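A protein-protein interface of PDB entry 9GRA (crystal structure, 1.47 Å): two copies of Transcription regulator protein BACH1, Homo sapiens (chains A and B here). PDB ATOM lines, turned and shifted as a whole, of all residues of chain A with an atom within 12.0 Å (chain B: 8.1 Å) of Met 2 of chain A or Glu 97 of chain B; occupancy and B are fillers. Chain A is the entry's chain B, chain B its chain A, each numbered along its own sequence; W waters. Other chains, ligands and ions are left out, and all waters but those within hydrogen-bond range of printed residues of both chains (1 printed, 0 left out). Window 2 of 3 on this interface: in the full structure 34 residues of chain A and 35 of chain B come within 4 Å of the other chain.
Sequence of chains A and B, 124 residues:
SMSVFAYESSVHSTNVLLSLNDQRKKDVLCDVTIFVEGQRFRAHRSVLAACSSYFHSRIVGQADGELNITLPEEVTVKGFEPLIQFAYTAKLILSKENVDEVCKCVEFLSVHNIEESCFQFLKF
The side-chain hydroxyl (OG) of Ser 95 of chain B lies close to the side-chain sulfur (SD) of Met 2 of chain A (3.7 Å). The side-chain sulfur (SD) of Met 2 of chain A is in hydrogen-bond range of the backbone NH (N) of Glu 97 of chain B (3.7 Å). The backbone NH (N) of Leu 94 of chain B sits at hydrogen-bond distance from the backbone carbonyl oxygen (O) of Phe 5 of chain A. N of Lys 96 of chain B is in hydrogen-bond range of O of Ser 3 of chain A (3.4 Å).
The side-chain amino group (NZ) of Lys 78 of chain B is in salt-bridge range of the side-chain carboxylate (OE2) of Glu 97 of chain B (3.2 Å). The side-chain hydroxyl (OG) of Ser 95 of chain B sits close to the backbone NH (N) of Glu 97 of chain B (3.2 Å). The backbone NH of Ser 95 of chain B lies within hydrogen-bond range of the side-chain amide oxygen of Asn 98 of chain B (2.8 Å).
Among the printed residues, merely in contact across the chains: Met 2 of chain A with Lys 96 of chain B, Ser 3 of chain A with Ser 95 of chain B, Ser 3 of chain A with Leu 122 of chain B, Val 4 of chain A with Leu 94 of chain B, Val 4 of chain A with Leu 122 of chain B and Phe 5 of chain A with Ile 93 of chain B.
Glu 97 of chain B touches one residue of chain A. Of chain A, only Met 2 (3.9 Å) and Ser 3 (3.4 Å) come within 4 Å of Lys 96 of chain B. No residue of chain A comes within 4 Å of Val 99 of chain B. No residue of chain A comes within 4 Å of Asp 100 of chain B. Of the printed residues of chain B, Phe 5 of chain A touches Ile 93 and Leu 94. Of the printed residues of chain A, Ile 93 of chain B touches Phe 5. Of the printed residues of chain A, Leu 122 of chain B touches Ser 3 (3.8 Å) and Val 4 (3.9 Å). Of the printed residues of chain B, Ser 3 of chain A touches Ser 95 (3.5 Å), Lys 96 (3.4 Å) and Leu 122 (3.8 Å). Of the printed residues of chain A, Leu 94 of chain B touches Val 4 (3.2 Å) and Phe 5 (2.8 Å). The nearest printed residue of chain B that does not touch Phe 5 of chain A is Leu 122 of chain B (4.005 Å).
Of the 16 printed residues of chain B, 6 touch a printed residue of chain A. Along chain B the printed residues that touch a printed residue of chain A span positions 93 to 122.
No position is printed for both chains.
Water W1 lies within hydrogen-bond range of O of Leu 122 of chain B (2.4 Å), O of Phe 124 of chain B (2.6 Å) and OG of Ser 3 of chain A (2.7 Å).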
ATOM      1  N   SER A   1      -9.910  16.957  14.153  1.00  0.00           N
ATOM      2  CA  SER A   1      -9.600  15.587  13.740  1.00  0.00           C
ATOM      3  C   SER A   1      -9.243  14.675  14.905  1.00  0.00           C
ATOM      4  O   SER A   1      -8.733  13.572  14.700  1.00  0.00           O
ATOM      5  CB  SER A   1      -8.453  15.556  12.736  1.00  0.00           C
ATOM      6  OG  SER A   1      -8.164  14.219  12.393  1.00  0.00           O
ATOM      7  N   MET A   2      -9.487  15.142  16.125  1.00  0.00           N
ATOM      8  CA  MET A   2      -9.492  14.286  17.299  1.00  0.00           C
ATOM      9  C   MET A   2     -10.948  14.112  17.727  1.00  0.00           C
ATOM     10  O   MET A   2     -11.730  15.065  17.693  1.00  0.00           O
ATOM     11  CB  MET A   2      -8.633  14.891  18.438  1.00  0.00           C
ATOM     12  CG  MET A   2      -8.522  14.044  19.756  1.00  0.00           C
ATOM     13  SD  MET A   2      -7.312  14.645  21.019  1.00  0.00           S
ATOM     14  CE  MET A   2      -5.897  15.003  19.973  1.00  0.00           C
ATOM     15  N   SER A   3     -11.309  12.894  18.122  1.00  0.00           N
ATOM     16  CA  SER A   3     -12.639  12.670  18.676  1.00  0.00           C
ATOM     17  C   SER A   3     -12.782  13.395  20.000  1.00  0.00           C
ATOM     18  O   SER A   3     -11.840  13.426  20.804  1.00  0.00           O
ATOM     19  CB  SER A   3     -12.826  11.188  18.959  1.00  0.00           C
ATOM     20  OG  SER A   3     -12.676  10.405  17.772  1.00  0.00           O
ATOM     21  N   VAL A   4     -13.973  13.940  20.243  1.00  0.00           N
ATOM     22  CA  VAL A   4     -14.224  14.709  21.448  1.00  0.00           C
ATOM     23  C   VAL A   4     -15.638  14.457  21.915  1.00  0.00           C
ATOM     24  O   VAL A   4     -16.556  14.246  21.104  1.00  0.00           O
ATOM     25  CB  VAL A   4     -14.038  16.223  21.234  1.00  0.00           C
ATOM     26  CG1 VAL A   4     -12.575  16.550  21.113  1.00  0.00           C
ATOM     27  CG2 VAL A   4     -14.799  16.686  19.995  1.00  0.00           C
ATOM     28  N   PHE A   5     -15.823  14.543  23.231  1.00  0.00           N
ATOM     29  CA  PHE A   5     -17.148  14.487  23.822  1.00  0.00           C
ATOM     30  C   PHE A   5     -17.278  15.657  24.772  1.00  0.00           C
ATOM     31  O   PHE A   5     -16.496  15.760  25.721  1.00  0.00           O
ATOM     32  CB  PHE A   5     -17.341  13.180  24.595  1.00  0.00           C
ATOM     33  CG  PHE A   5     -18.737  12.982  25.084  1.00  0.00           C
ATOM     34  CD1 PHE A   5     -19.157  13.525  26.298  1.00  0.00           C
ATOM     35  CD2 PHE A   5     -19.634  12.241  24.343  1.00  0.00           C
ATOM     36  CE1 PHE A   5     -20.474  13.331  26.737  1.00  0.00           C
ATOM     37  CE2 PHE A   5     -20.951  12.027  24.781  1.00  0.00           C
ATOM     38  CZ  PHE A   5     -21.367  12.571  25.986  1.00  0.00           C
ATOM     39  N   ALA A   6     -18.252  16.534  24.515  1.00  0.00           N
ATOM     40  CA  ALA A   6     -18.392  17.758  25.280  1.00  0.00           C
ATOM     41  C   ALA A   6     -19.716  17.773  26.027  1.00  0.00           C
ATOM     42  O   ALA A   6     -20.741  17.333  25.492  1.00  0.00           O
ATOM     43  CB  ALA A   6     -18.321  18.971  24.357  1.00  0.00           C
ATOM     44  N   THR B  76      -2.101  16.351  36.347  1.00  0.00           N
ATOM     45  CA  THR B  76      -1.376  16.794  35.172  1.00  0.00           C
ATOM     46  C   THR B  76      -2.104  17.976  34.558  1.00  0.00           C
ATOM     47  O   THR B  76      -3.321  18.158  34.748  1.00  0.00           O
ATOM     48  CB  THR B  76      -1.271  15.661  34.161  1.00  0.00           C
ATOM     49  OG1 THR B  76      -2.583  15.346  33.723  1.00  0.00           O
ATOM     50  CG2 THR B  76      -0.612  14.383  34.797  1.00  0.00           C
ATOM     51  N   LYS B  78      -2.775  18.213  31.504  1.00  0.00           N
ATOM     52  CA  LYS B  78      -3.742  17.580  30.607  1.00  0.00           C
ATOM     53  C   LYS B  78      -5.073  17.341  31.294  1.00  0.00           C
ATOM     54  O   LYS B  78      -6.141  17.508  30.682  1.00  0.00           O
ATOM     55  CB  LYS B  78      -3.143  16.260  30.112  1.00  0.00           C
ATOM     56  CG  LYS B  78      -3.864  15.647  28.967  1.00  0.00           C
ATOM     57  CD  LYS B  78      -3.033  14.529  28.320  1.00  0.00           C
ATOM     58  CE  LYS B  78      -1.773  15.089  27.675  1.00  0.00           C
ATOM     59  NZ  LYS B  78      -0.977  14.020  27.001  1.00  0.00           N
ATOM     60  N   GLY B  79      -5.034  16.885  32.533  1.00  0.00           N
ATOM     61  CA  GLY B  79      -6.251  16.551  33.246  1.00  0.00           C
ATOM     62  C   GLY B  79      -6.890  17.758  33.924  1.00  0.00           C
ATOM     63  O   GLY B  79      -8.105  17.839  34.056  1.00  0.00           O
ATOM     64  N   ILE B  93     -14.745  19.540  27.910  1.00  0.00           N
ATOM     65  CA  ILE B  93     -14.404  18.875  26.656  1.00  0.00           C
ATOM     66  C   ILE B  93     -13.481  17.700  26.954  1.00  0.00           C
ATOM     67  O   ILE B  93     -12.360  17.905  27.440  1.00  0.00           O
ATOM     68  CB  ILE B  93     -13.746  19.858  25.688  1.00  0.00           C
ATOM     69  CG1 ILE B  93     -14.696  20.998  25.349  1.00  0.00           C
ATOM     70  CG2 ILE B  93     -13.385  19.146  24.421  1.00  0.00           C
ATOM     71  CD1 ILE B  93     -14.115  21.925  24.318  1.00  0.00           C
ATOM     72  N   LEU B  94     -13.940  16.454  26.673  1.00  0.00           N
ATOM     73  CA  LEU B  94     -13.105  15.256  26.818  1.00  0.00           C
ATOM     74  C   LEU B  94     -12.582  14.840  25.445  1.00  0.00           C
ATOM     75  O   LEU B  94     -13.308  14.908  24.458  1.00  0.00           O
ATOM     76  CB  LEU B  94     -13.887  14.096  27.432  1.00  0.00           C
ATOM     77  CG  LEU B  94     -14.620  14.361  28.738  1.00  0.00           C
ATOM     78  CD1 LEU B  94     -15.400  13.116  29.156  1.00  0.00           C
ATOM     79  CD2 LEU B  94     -13.612  14.777  29.828  1.00  0.00           C
ATOM     80  N   SER B  95     -11.314  14.446  25.370  1.00  0.00           N
ATOM     81  CA  SER B  95     -10.722  14.052  24.102  1.00  0.00           C
ATOM     82  C   SER B  95     -10.052  12.712  24.255  1.00  0.00           C
ATOM     83  O   SER B  95      -9.774  12.247  25.360  1.00  0.00           O
ATOM     84  CB  SER B  95      -9.646  15.035  23.628  1.00  0.00           C
ATOM     85  OG  SER B  95      -8.551  14.987  24.533  1.00  0.00           O
ATOM     86  N   LYS B  96      -9.752  12.119  23.110  1.00  0.00           N
ATOM     87  CA  LYS B  96      -8.959  10.903  23.118  1.00  0.00           C
ATOM     88  C   LYS B  96      -7.713  11.095  23.964  1.00  0.00           C
ATOM     89  O   LYS B  96      -7.349  10.235  24.767  1.00  0.00           O
ATOM     90  CB  LYS B  96      -8.521  10.604  21.694  1.00  0.00           C
ATOM     91  CG  LYS B  96      -7.509   9.474  21.632  1.00  0.00           C
ATOM     92  CD  LYS B  96      -7.358   8.967  20.197  1.00  0.00           C
ATOM     93  CE  LYS B  96      -6.198   8.026  20.021  1.00  0.00           C
ATOM     94  NZ  LYS B  96      -6.066   7.695  18.567  1.00  0.00           N
ATOM     95  N   GLU B  97      -7.059  12.232  23.801  1.00  0.00           N
ATOM     96  CA  GLU B  97      -5.793  12.461  24.500  1.00  0.00           C
ATOM     97  C   GLU B  97      -5.974  12.705  26.000  1.00  0.00           C
ATOM     98  O   GLU B  97      -5.092  12.333  26.790  1.00  0.00           O
ATOM     99  CB  GLU B  97      -5.080  13.632  23.831  1.00  0.00           C
ATOM    100  CG  GLU B  97      -3.876  14.147  24.574  1.00  0.00           C
ATOM    101  CD  GLU B  97      -2.918  14.923  23.680  1.00  0.00           C
ATOM    102  OE1 GLU B  97      -3.304  15.262  22.534  1.00  0.00           O
ATOM    103  OE2 GLU B  97      -1.776  15.183  24.122  1.00  0.00           O
ATOM    104  N   ASN B  98      -7.093  13.301  26.439  1.00  0.00           N
ATOM    105  CA  ASN B  98      -7.089  13.727  27.830  1.00  0.00           C
ATOM    106  C   ASN B  98      -8.042  12.968  28.730  1.00  0.00           C
ATOM    107  O   ASN B  98      -8.050  13.239  29.936  1.00  0.00           O
ATOM    108  CB  ASN B  98      -7.347  15.238  27.966  1.00  0.00           C
ATOM    109  CG  ASN B  98      -8.779  15.627  27.623  1.00  0.00           C
ATOM    110  OD1 ASN B  98      -9.692  14.780  27.634  1.00  0.00           O
ATOM    111  ND2 ASN B  98      -8.997  16.921  27.369  1.00  0.00           N
ATOM    112  N   VAL B  99      -8.867  12.069  28.179  1.00  0.00           N
ATOM    113  CA  VAL B  99     -10.021  11.586  28.939  1.00  0.00           C
ATOM    114  C   VAL B  99      -9.594  10.890  30.230  1.00  0.00           C
ATOM    115  O   VAL B  99     -10.178  11.132  31.301  1.00  0.00           O
ATOM    116  CB  VAL B  99     -10.953  10.717  28.067  1.00  0.00           C
ATOM    117  CG1 VAL B  99     -10.223   9.536  27.443  1.00  0.00           C
ATOM    118  CG2 VAL B  99     -12.148  10.274  28.927  1.00  0.00           C
ATOM    119  N   ASP B 100      -8.545  10.057  30.176  1.00  0.00           N
ATOM    120  CA  ASP B 100      -8.201   9.322  31.390  1.00  0.00           C
ATOM    121  C   ASP B 100      -7.709  10.286  32.454  1.00  0.00           C
ATOM    122  O   ASP B 100      -8.037  10.143  33.631  1.00  0.00           O
ATOM    123  CB  ASP B 100      -7.132   8.254  31.095  1.00  0.00           C
ATOM    124  CG  ASP B 100      -7.631   7.107  30.223  1.00  0.00           C
ATOM    125  OD1 ASP B 100      -8.850   6.908  30.068  1.00  0.00           O
ATOM    126  OD2 ASP B 100      -6.775   6.356  29.697  1.00  0.00           O
ATOM    127  N   GLU B 101      -6.871  11.258  32.064  1.00  0.00           N
ATOM    128  CA  GLU B 101      -6.336  12.198  33.035  1.00  0.00           C
ATOM    129  C   GLU B 101      -7.436  13.093  33.613  1.00  0.00           C
ATOM    130  O   GLU B 101      -7.397  13.449  34.801  1.00  0.00           O
ATOM    131  CB  GLU B 101      -5.218  13.046  32.408  1.00  0.00           C
ATOM    132  CG  GLU B 101      -3.930  12.260  32.070  1.00  0.00           C
ATOM    133  CD  GLU B 101      -3.415  11.447  33.245  1.00  0.00           C
ATOM    134  OE1 GLU B 101      -3.199  12.044  34.328  1.00  0.00           O
ATOM    135  OE2 GLU B 101      -3.231  10.219  33.096  1.00  0.00           O
ATOM    136  N   VAL B 102      -8.394  13.523  32.780  1.00  0.00           N
ATOM    137  CA  VAL B 102      -9.460  14.368  33.316  1.00  0.00           C
ATOM    138  C   VAL B 102     -10.259  13.569  34.319  1.00  0.00           C
ATOM    139  O   VAL B 102     -10.662  14.084  35.367  1.00  0.00           O
ATOM    140  CB  VAL B 102     -10.360  14.882  32.177  1.00  0.00           C
ATOM    141  CG1 VAL B 102     -11.607  15.553  32.710  1.00  0.00           C
ATOM    142  CG2 VAL B 102      -9.607  15.851  31.329  1.00  0.00           C
ATOM    143  N   LEU B 122     -13.599   7.153  22.854  1.00  0.00           N
ATOM    144  CA  LEU B 122     -12.839   8.301  22.369  1.00  0.00           C
ATOM    145  C   LEU B 122     -11.484   7.889  21.838  1.00  0.00           C
ATOM    146  O   LEU B 122     -10.888   8.626  21.047  1.00  0.00           O
ATOM    147  CB  LEU B 122     -12.671   9.346  23.468  1.00  0.00           C
ATOM    148  CG  LEU B 122     -13.954  10.042  23.867  1.00  0.00           C
ATOM    149  CD1 LEU B 122     -13.635  11.005  24.998  1.00  0.00           C
ATOM    150  CD2 LEU B 122     -14.467  10.818  22.661  1.00  0.00           C
ATOM    151  N   LYS B 123     -10.999   6.719  22.239  1.00  0.00           N
ATOM    152  CA  LYS B 123      -9.701   6.208  21.821  1.00  0.00           C
ATOM    153  C   LYS B 123      -9.736   5.434  20.513  1.00  0.00           C
ATOM    154  O   LYS B 123      -8.674   5.042  20.019  1.00  0.00           O
ATOM    155  CB  LYS B 123      -9.111   5.347  22.939  1.00  0.00           C
ATOM    156  CG  LYS B 123      -8.609   6.214  24.075  1.00  0.00           C
ATOM    157  CD  LYS B 123      -8.067   5.391  25.244  1.00  0.00           C
ATOM    158  CE  LYS B 123      -8.063   6.215  26.522  1.00  0.00           C
ATOM    159  NZ  LYS B 123      -7.687   5.411  27.708  1.00  0.00           N
ATOM    160  N   PHE B 124     -10.910   5.209  19.931  1.00  0.00           N
ATOM    161  CA  PHE B 124     -10.965   4.428  18.695  1.00  0.00           C
ATOM    162  C   PHE B 124     -10.381   5.229  17.538  1.00  0.00           C
ATOM    163  O   PHE B 124     -10.042   6.403  17.701  1.00  0.00           O
ATOM    164  CB  PHE B 124     -12.391   3.980  18.392  1.00  0.00           C
ATOM    165  CG  PHE B 124     -12.945   3.037  19.409  1.00  0.00           C
ATOM    166  CD1 PHE B 124     -12.094   2.383  20.299  1.00  0.00           C
ATOM    167  CD2 PHE B 124     -14.314   2.804  19.489  1.00  0.00           C
ATOM    168  CE1 PHE B 124     -12.597   1.517  21.257  1.00  0.00           C
ATOM    169  CE2 PHE B 124     -14.828   1.935  20.439  1.00  0.00           C
ATOM    170  CZ  PHE B 124     -13.964   1.286  21.326  1.00  0.00           C
HETATM  171  O   HOH W   1     -10.692   8.729  18.652  1.00  0.00           O
